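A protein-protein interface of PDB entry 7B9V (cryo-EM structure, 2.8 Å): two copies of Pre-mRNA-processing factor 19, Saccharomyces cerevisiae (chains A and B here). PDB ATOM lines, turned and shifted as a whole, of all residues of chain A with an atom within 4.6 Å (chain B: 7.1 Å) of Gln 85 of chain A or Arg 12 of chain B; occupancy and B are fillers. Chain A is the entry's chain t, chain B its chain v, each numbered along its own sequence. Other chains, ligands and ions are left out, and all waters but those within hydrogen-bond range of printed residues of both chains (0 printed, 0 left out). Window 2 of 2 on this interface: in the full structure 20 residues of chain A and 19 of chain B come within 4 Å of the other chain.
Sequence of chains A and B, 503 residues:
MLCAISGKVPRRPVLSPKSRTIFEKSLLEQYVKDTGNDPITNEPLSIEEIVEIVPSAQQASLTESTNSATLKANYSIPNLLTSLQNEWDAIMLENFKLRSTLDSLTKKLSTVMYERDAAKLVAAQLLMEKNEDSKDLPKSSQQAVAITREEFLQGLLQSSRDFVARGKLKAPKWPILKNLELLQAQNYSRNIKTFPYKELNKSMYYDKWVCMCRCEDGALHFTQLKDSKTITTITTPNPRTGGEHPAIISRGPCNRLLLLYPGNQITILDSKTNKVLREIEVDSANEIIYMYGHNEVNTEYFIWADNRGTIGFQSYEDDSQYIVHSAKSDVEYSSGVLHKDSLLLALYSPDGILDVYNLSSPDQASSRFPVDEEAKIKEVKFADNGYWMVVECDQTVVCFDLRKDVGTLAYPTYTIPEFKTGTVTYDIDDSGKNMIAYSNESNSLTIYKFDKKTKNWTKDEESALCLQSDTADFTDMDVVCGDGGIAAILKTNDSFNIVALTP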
ATOM      1  N   LEU A  81      -8.771   1.146  -0.590  1.00  0.00           N
ATOM      2  CA  LEU A  81      -9.195  -0.176  -0.113  1.00  0.00           C
ATOM      3  C   LEU A  81     -10.100  -0.870  -1.137  1.00  0.00           C
ATOM      4  O   LEU A  81      -9.960  -2.076  -1.348  1.00  0.00           O
ATOM      5  CB  LEU A  81      -9.891  -0.043   1.243  1.00  0.00           C
ATOM      6  CG  LEU A  81      -8.981   0.236   2.436  1.00  0.00           C
ATOM      7  CD1 LEU A  81      -9.784   0.684   3.646  1.00  0.00           C
ATOM      8  CD2 LEU A  81      -8.195  -1.015   2.764  1.00  0.00           C
ATOM      9  N   THR A  82     -11.078  -0.162  -1.711  1.00  0.00           N
ATOM     10  CA  THR A  82     -11.955  -0.722  -2.753  1.00  0.00           C
ATOM     11  C   THR A  82     -11.140  -1.158  -3.975  1.00  0.00           C
ATOM     12  O   THR A  82     -11.331  -2.266  -4.494  1.00  0.00           O
ATOM     13  CB  THR A  82     -13.021   0.294  -3.191  1.00  0.00           C
ATOM     14  OG1 THR A  82     -13.811   0.690  -2.071  1.00  0.00           O
ATOM     15  CG2 THR A  82     -13.935  -0.305  -4.280  1.00  0.00           C
ATOM     16  N   SER A  83     -10.265  -0.275  -4.465  1.00  0.00           N
ATOM     17  CA  SER A  83      -9.372  -0.559  -5.589  1.00  0.00           C
ATOM     18  C   SER A  83      -8.477  -1.754  -5.288  1.00  0.00           C
ATOM     19  O   SER A  83      -8.525  -2.728  -6.026  1.00  0.00           O
ATOM     20  CB  SER A  83      -8.521   0.670  -5.919  1.00  0.00           C
ATOM     21  N   LEU A  84      -7.773  -1.743  -4.151  1.00  0.00           N
ATOM     22  CA  LEU A  84      -6.905  -2.835  -3.691  1.00  0.00           C
ATOM     23  C   LEU A  84      -7.664  -4.149  -3.491  1.00  0.00           C
ATOM     24  O   LEU A  84      -7.133  -5.222  -3.783  1.00  0.00           O
ATOM     25  CB  LEU A  84      -6.218  -2.435  -2.388  1.00  0.00           C
ATOM     26  CG  LEU A  84      -5.280  -3.443  -1.725  1.00  0.00           C
ATOM     27  CD1 LEU A  84      -4.112  -3.799  -2.637  1.00  0.00           C
ATOM     28  CD2 LEU A  84      -4.801  -2.849  -0.428  1.00  0.00           C
ATOM     29  N   GLN A  85      -8.900  -4.086  -2.999  1.00  0.00           N
ATOM     30  CA  GLN A  85      -9.762  -5.262  -2.865  1.00  0.00           C
ATOM     31  C   GLN A  85     -10.180  -5.816  -4.230  1.00  0.00           C
ATOM     32  O   GLN A  85     -10.208  -7.030  -4.416  1.00  0.00           O
ATOM     33  CB  GLN A  85     -10.984  -4.903  -1.994  1.00  0.00           C
ATOM     34  CG  GLN A  85     -12.030  -6.020  -1.702  1.00  0.00           C
ATOM     35  CD  GLN A  85     -13.071  -6.232  -2.813  1.00  0.00           C
ATOM     36  OE1 GLN A  85     -13.440  -5.297  -3.510  1.00  0.00           O
ATOM     37  NE2 GLN A  85     -13.468  -7.479  -3.016  1.00  0.00           N
ATOM     38  N   ASN A  86     -10.499  -4.949  -5.192  1.00  0.00           N
ATOM     39  CA  ASN A  86     -10.818  -5.338  -6.579  1.00  0.00           C
ATOM     40  C   ASN A  86      -9.576  -5.785  -7.360  1.00  0.00           C
ATOM     41  O   ASN A  86      -9.662  -6.680  -8.209  1.00  0.00           O
ATOM     42  CB  ASN A  86     -11.524  -4.186  -7.292  1.00  0.00           C
ATOM     43  CG  ASN A  86     -12.876  -3.879  -6.685  1.00  0.00           C
ATOM     44  N   GLU A  87      -8.425  -5.221  -7.032  1.00  0.00           N
ATOM     45  CA  GLU A  87      -7.125  -5.680  -7.512  1.00  0.00           C
ATOM     46  C   GLU A  87      -6.808  -7.045  -6.938  1.00  0.00           C
ATOM     47  O   GLU A  87      -6.395  -7.926  -7.681  1.00  0.00           O
ATOM     48  CB  GLU A  87      -6.005  -4.685  -7.171  1.00  0.00           C
ATOM     49  CG  GLU A  87      -6.049  -3.359  -7.901  1.00  0.00           C
ATOM     50  CD  GLU A  87      -5.341  -2.259  -7.137  1.00  0.00           C
ATOM     51  OE1 GLU A  87      -4.275  -2.515  -6.534  1.00  0.00           O
ATOM     52  OE2 GLU A  87      -5.879  -1.131  -7.121  1.00  0.00           O
ATOM     53  N   TRP A  88      -7.015  -7.237  -5.635  1.00  0.00           N
ATOM     54  CA  TRP A  88      -6.935  -8.564  -5.006  1.00  0.00           C
ATOM     55  C   TRP A  88      -7.934  -9.536  -5.637  1.00  0.00           C
ATOM     56  O   TRP A  88      -7.587 -10.698  -5.821  1.00  0.00           O
ATOM     57  CB  TRP A  88      -7.156  -8.461  -3.491  1.00  0.00           C
ATOM     58  CG  TRP A  88      -7.168  -9.799  -2.760  1.00  0.00           C
ATOM     59  CD1 TRP A  88      -6.074 -10.479  -2.311  1.00  0.00           C
ATOM     60  CD2 TRP A  88      -8.312 -10.580  -2.370  1.00  0.00           C
ATOM     61  NE1 TRP A  88      -6.450 -11.636  -1.682  1.00  0.00           N
ATOM     62  CE2 TRP A  88      -7.815 -11.721  -1.699  1.00  0.00           C
ATOM     63  CE3 TRP A  88      -9.687 -10.434  -2.525  1.00  0.00           C
ATOM     64  CZ2 TRP A  88      -8.656 -12.708  -1.195  1.00  0.00           C
ATOM     65  CZ3 TRP A  88     -10.518 -11.407  -2.019  1.00  0.00           C
ATOM     66  CH2 TRP A  88      -9.999 -12.528  -1.362  1.00  0.00           C
ATOM     67  N   ASP A  89      -9.174  -9.108  -5.912  1.00  0.00           N
ATOM     68  CA  ASP A  89     -10.134  -9.925  -6.677  1.00  0.00           C
ATOM     69  C   ASP A  89      -9.555 -10.369  -8.026  1.00  0.00           C
ATOM     70  O   ASP A  89      -9.625 -11.552  -8.377  1.00  0.00           O
ATOM     71  CB  ASP A  89     -11.482  -9.228  -6.953  1.00  0.00           C
ATOM     72  CG  ASP A  89     -12.284  -8.896  -5.712  1.00  0.00           C
ATOM     73  OD1 ASP A  89     -12.174  -9.616  -4.701  1.00  0.00           O
ATOM     74  OD2 ASP A  89     -13.090  -7.940  -5.782  1.00  0.00           O
ATOM     75  N   VAL B   9     -11.005 -18.443   4.719  1.00  0.00           N
ATOM     76  CA  VAL B   9     -12.421 -18.306   5.090  1.00  0.00           C
ATOM     77  C   VAL B   9     -13.008 -17.101   4.366  1.00  0.00           C
ATOM     78  O   VAL B   9     -12.379 -16.030   4.366  1.00  0.00           O
ATOM     79  CB  VAL B   9     -12.552 -18.148   6.603  1.00  0.00           C
ATOM     80  CG1 VAL B   9     -14.012 -17.995   7.002  1.00  0.00           C
ATOM     81  CG2 VAL B   9     -11.922 -19.333   7.318  1.00  0.00           C
ATOM     82  N   PRO B  10     -14.136 -17.250   3.662  1.00  0.00           N
ATOM     83  CA  PRO B  10     -14.785 -16.104   3.018  1.00  0.00           C
ATOM     84  C   PRO B  10     -15.195 -14.987   3.976  1.00  0.00           C
ATOM     85  O   PRO B  10     -15.586 -15.223   5.119  1.00  0.00           O
ATOM     86  CB  PRO B  10     -16.026 -16.708   2.338  1.00  0.00           C
ATOM     87  CG  PRO B  10     -15.700 -18.133   2.097  1.00  0.00           C
ATOM     88  CD  PRO B  10     -14.820 -18.481   3.317  1.00  0.00           C
ATOM     89  N   ARG B  11     -15.120 -13.750   3.479  1.00  0.00           N
ATOM     90  CA  ARG B  11     -15.784 -12.632   4.141  1.00  0.00           C
ATOM     91  C   ARG B  11     -17.289 -12.634   3.901  1.00  0.00           C
ATOM     92  O   ARG B  11     -18.084 -12.314   4.795  1.00  0.00           O
ATOM     93  CB  ARG B  11     -15.175 -11.331   3.633  1.00  0.00           C
ATOM     94  CG  ARG B  11     -13.679 -11.173   3.908  1.00  0.00           C
ATOM     95  CD  ARG B  11     -13.310 -10.656   5.315  1.00  0.00           C
ATOM     96  NE  ARG B  11     -13.680 -11.500   6.456  1.00  0.00           N
ATOM     97  CZ  ARG B  11     -13.020 -12.583   6.846  1.00  0.00           C
ATOM     98  NH1 ARG B  11     -12.009 -13.072   6.139  1.00  0.00           N
ATOM     99  NH2 ARG B  11     -13.422 -13.226   7.940  1.00  0.00           N
ATOM    100  N   ARG B  12     -17.679 -13.013   2.689  1.00  0.00           N
ATOM    101  CA  ARG B  12     -19.066 -13.055   2.223  1.00  0.00           C
ATOM    102  C   ARG B  12     -19.238 -14.385   1.505  1.00  0.00           C
ATOM    103  O   ARG B  12     -19.036 -14.470   0.291  1.00  0.00           O
ATOM    104  CB  ARG B  12     -19.336 -11.868   1.290  1.00  0.00           C
ATOM    105  CG  ARG B  12     -19.160 -10.491   1.942  1.00  0.00           C
ATOM    106  CD  ARG B  12     -18.967  -9.370   0.956  1.00  0.00           C
ATOM    107  NE  ARG B  12     -17.758  -9.655   0.181  1.00  0.00           N
ATOM    108  CZ  ARG B  12     -17.170  -8.812  -0.652  1.00  0.00           C
ATOM    109  NH1 ARG B  12     -17.633  -7.584  -0.840  1.00  0.00           N
ATOM    110  NH2 ARG B  12     -16.064  -9.199  -1.280  1.00  0.00           N
ATOM    111  N   PRO B  13     -19.524 -15.454   2.246  1.00  0.00           N
ATOM    112  CA  PRO B  13     -19.581 -16.782   1.623  1.00  0.00           C
ATOM    113  C   PRO B  13     -20.745 -16.986   0.664  1.00  0.00           C
ATOM    114  O   PRO B  13     -21.877 -16.581   0.929  1.00  0.00           O
ATOM    115  CB  PRO B  13     -19.685 -17.758   2.813  1.00  0.00           C
ATOM    116  CG  PRO B  13     -20.307 -16.983   3.898  1.00  0.00           C
ATOM    117  CD  PRO B  13     -19.765 -15.556   3.673  1.00  0.00           C
ATOM    118  N   VAL B  14     -20.454 -17.653  -0.455  1.00  0.00           N
ATOM    119  CA  VAL B  14     -21.456 -18.041  -1.443  1.00  0.00           C
ATOM    120  C   VAL B  14     -21.192 -19.453  -1.968  1.00  0.00           C
ATOM    121  O   VAL B  14     -20.071 -19.967  -1.891  1.00  0.00           O
ATOM    122  CB  VAL B  14     -21.563 -17.045  -2.638  1.00  0.00           C
ATOM    123  CG1 VAL B  14     -21.689 -15.560  -2.280  1.00  0.00           C
ATOM    124  CG2 VAL B  14     -20.318 -17.148  -3.500  1.00  0.00           C
ATOM    125  N   LEU B  15     -22.263 -20.105  -2.431  1.00  0.00           N
ATOM    126  CA  LEU B  15     -22.193 -21.402  -3.104  1.00  0.00           C
ATOM    127  C   LEU B  15     -22.649 -21.294  -4.555  1.00  0.00           C
ATOM    128  O   LEU B  15     -23.726 -20.754  -4.821  1.00  0.00           O
ATOM    129  CB  LEU B  15     -23.012 -22.470  -2.356  1.00  0.00           C
ATOM    130  CG  LEU B  15     -23.189 -23.863  -2.976  1.00  0.00           C
ATOM    131  CD1 LEU B  15     -22.961 -24.921  -1.935  1.00  0.00           C
ATOM    132  CD2 LEU B  15     -24.621 -24.019  -3.477  1.00  0.00           C
ATOM    133  N   PHE B  23     -17.345 -20.344  -2.136  1.00  0.00           N
ATOM    134  CA  PHE B  23     -16.535 -19.275  -2.700  1.00  0.00           C
ATOM    135  C   PHE B  23     -16.704 -18.020  -1.847  1.00  0.00           C
ATOM    136  O   PHE B  23     -17.676 -17.879  -1.103  1.00  0.00           O
ATOM    137  CB  PHE B  23     -16.922 -18.968  -4.165  1.00  0.00           C
ATOM    138  CG  PHE B  23     -16.878 -20.168  -5.089  1.00  0.00           C
ATOM    139  CD1 PHE B  23     -15.691 -20.507  -5.712  1.00  0.00           C
ATOM    140  CD2 PHE B  23     -18.003 -20.949  -5.329  1.00  0.00           C
ATOM    141  CE1 PHE B  23     -15.606 -21.587  -6.568  1.00  0.00           C
ATOM    142  CE2 PHE B  23     -17.928 -22.048  -6.190  1.00  0.00           C
ATOM    143  CZ  PHE B  23     -16.726 -22.359  -6.807  1.00  0.00           C
ATOM    144  N   GLU B  24     -15.731 -17.108  -1.969  1.00  0.00           N
ATOM    145  CA  GLU B  24     -15.901 -15.692  -1.644  1.00  0.00           C
ATOM    146  C   GLU B  24     -16.702 -15.027  -2.755  1.00  0.00           C
ATOM    147  O   GLU B  24     -16.443 -15.297  -3.932  1.00  0.00           O
ATOM    148  CB  GLU B  24     -14.544 -14.997  -1.486  1.00  0.00           C
ATOM    149  CG  GLU B  24     -14.575 -13.457  -1.360  1.00  0.00           C
ATOM    150  CD  GLU B  24     -15.563 -12.910  -0.321  1.00  0.00           C
ATOM    151  OE1 GLU B  24     -15.706 -13.501   0.776  1.00  0.00           O
ATOM    152  OE2 GLU B  24     -16.210 -11.885  -0.613  1.00  0.00           O
ATOM    153  N   LYS B  25     -17.734 -14.251  -2.362  1.00  0.00           N
ATOM    154  CA  LYS B  25     -18.674 -13.544  -3.239  1.00  0.00           C
ATOM    155  C   LYS B  25     -18.034 -12.845  -4.437  1.00  0.00           C
ATOM    156  O   LYS B  25     -18.360 -13.178  -5.579  1.00  0.00           O
ATOM    157  CB  LYS B  25     -19.479 -12.531  -2.402  1.00  0.00           C
ATOM    158  CG  LYS B  25     -20.486 -11.638  -3.172  1.00  0.00           C
ATOM    159  CD  LYS B  25     -21.065 -10.548  -2.257  1.00  0.00           C
ATOM    160  CE  LYS B  25     -21.881  -9.506  -3.016  1.00  0.00           C
ATOM    161  NZ  LYS B  25     -23.099 -10.079  -3.666  1.00  0.00           N
ATOM    162  N   SER B  26     -17.157 -11.859  -4.191  1.00  0.00           N
ATOM    163  CA  SER B  26     -16.587 -11.045  -5.271  1.00  0.00           C
ATOM    164  C   SER B  26     -15.740 -11.861  -6.252  1.00  0.00           C
ATOM    165  O   SER B  26     -15.730 -11.564  -7.447  1.00  0.00           O
ATOM    166  CB  SER B  26     -15.762  -9.898  -4.691  1.00  0.00           C
ATOM    167  OG  SER B  26     -16.581  -8.963  -4.007  1.00  0.00           O
ATOM    168  N   LEU B  27     -15.113 -12.948  -5.783  1.00  0.00           N
ATOM    169  CA  LEU B  27     -14.314 -13.816  -6.649  1.00  0.00           C
ATOM    170  C   LEU B  27     -15.190 -14.611  -7.628  1.00  0.00           C
ATOM    171  O   LEU B  27     -14.953 -14.595  -8.853  1.00  0.00           O
ATOM    172  CB  LEU B  27     -13.467 -14.729  -5.750  1.00  0.00           C
ATOM    173  CG  LEU B  27     -12.547 -13.999  -4.752  1.00  0.00           C
ATOM    174  CD1 LEU B  27     -11.648 -14.895  -3.890  1.00  0.00           C
ATOM    175  CD2 LEU B  27     -11.657 -13.082  -5.530  1.00  0.00           C
ATOM    176  N   GLN B  30     -16.938 -12.139  -9.997  1.00  0.00           N
ATOM    177  CA  GLN B  30     -16.013 -11.650 -11.025  1.00  0.00           C
ATOM    178  C   GLN B  30     -15.856 -12.661 -12.160  1.00  0.00           C
ATOM    179  O   GLN B  30     -15.836 -12.275 -13.339  1.00  0.00           O
ATOM    180  CB  GLN B  30     -14.659 -11.254 -10.431  1.00  0.00           C
ATOM    181  CG  GLN B  30     -13.854 -10.367 -11.402  1.00  0.00           C
ATOM    182  CD  GLN B  30     -12.487  -9.975 -10.860  1.00  0.00           C
ATOM    183  OE1 GLN B  30     -11.934 -10.663 -10.019  1.00  0.00           O
ATOM    184  NE2 GLN B  30     -11.954  -8.862 -11.345  1.00  0.00           N
ATOM    185  N   GLU B  52     -25.883 -17.040  -2.321  1.00  0.00           N
ATOM    186  CA  GLU B  52     -25.401 -16.322  -1.146  1.00  0.00           C
ATOM    187  C   GLU B  52     -25.822 -17.066   0.121  1.00  0.00           C
ATOM    188  O   GLU B  52     -26.945 -17.571   0.216  1.00  0.00           O
ATOM    189  CB  GLU B  52     -25.986 -14.912  -1.162  1.00  0.00           C
ATOM    190  CG  GLU B  52     -25.263 -13.929  -2.098  1.00  0.00           C
ATOM    191  CD  GLU B  52     -24.472 -12.863  -1.376  1.00  0.00           C
ATOM    192  OE1 GLU B  52     -23.907 -13.153  -0.301  1.00  0.00           O
ATOM    193  OE2 GLU B  52     -24.421 -11.726  -1.897  1.00  0.00           O
ATOM    194  N   ILE B  53     -24.934 -17.113   1.106  1.00  0.00           N
ATOM    195  CA  ILE B  53     -25.151 -17.888   2.324  1.00  0.00           C
ATOM    196  C   ILE B  53     -25.391 -16.965   3.514  1.00  0.00           C
ATOM    197  O   ILE B  53     -24.541 -16.128   3.841  1.00  0.00           O
ATOM    198  CB  ILE B  53     -23.977 -18.843   2.577  1.00  0.00           C
ATOM    199  CG1 ILE B  53     -23.873 -19.838   1.419  1.00  0.00           C
ATOM    200  CG2 ILE B  53     -24.153 -19.526   3.886  1.00  0.00           C
ATOM    201  CD1 ILE B  53     -22.681 -20.753   1.494  1.00  0.00           C
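Printed residues of chain B within 4 Å of Gln 85 of chain A: Arg 12 and Ser 26.
Of the printed residues of chain B, Trp 88 of chain A touches Leu 27.
Of the printed residues of chain B, Asp 89 of chain A touches Ser 26 (3.5 Å), Leu 27 (3.6 Å) and Gln 30 (3.0 Å).
Of chain A, only Gln 85 comes within 4 Å of Arg 12 of chain B.
Printed residues of chain A within 4 Å of Ser 26 of chain B: Gln 85 (3.6 Å) and Asp 89 (3.5 Å).
Printed residues of chain A within 4 Å of Leu 27 of chain B: Trp 88 (3.8 Å) and Asp 89 (3.6 Å).
The nearest printed residue of chain A that does not touch Arg 12 of chain B is Asp 89 of chain A (5.2 Å).
The nearest printed residue of chain A that does not touch Leu 27 of chain B is Gln 85 of chain A (6.3 Å).
Gln 85 of chain A touches Arg 12 of chain B.
Gln 85 of chain A touches Ser 26 of chain B (NE2 to OG, 3.6 Å).
Trp 88 of chain A touches Leu 27 of chain B.
Asp 89 of chain A touches Ser 26 of chain B (OD2 to CB, 3.5 Å).
Asp 89 of chain A touches Leu 27 of chain B.
No position is printed for both chains.
Hydrophobic or aromatic side chains of chain B within 4 Å of the printed part of chain A: Leu 27.
Among the printed residues, 6 pairs touch across the chains.
The backbone carbonyl oxygen (O) of Asp 89 of chain A sits close to the side-chain amide oxygen (OE1) of Gln 30 of chain B, 3.0 Å away.
The backbone NH of Lys 25 of chain B lies within hydrogen-bond range of the backbone carbonyl oxygen of Arg 12 of chain B (3.0 Å).
The side-chain amide nitrogen (NE2) of Gln 85 of chain A sits at hydrogen-bond distance from the side-chain carboxylate (OD2) of Asp 89 of chain A, at 2.8 Å.
The guanidinium group (NH2) of Arg 12 of chain B is in salt-bridge range of the side-chain carboxylate (OE2) of Glu 24 of chain B, at 2.8 Å.
The side-chain hydroxyl (OG) of Ser 26 of chain B sits at hydrogen-bond distance from the guanidinium group (NH2) of Arg 12 of chain B, at 2.8 Å.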
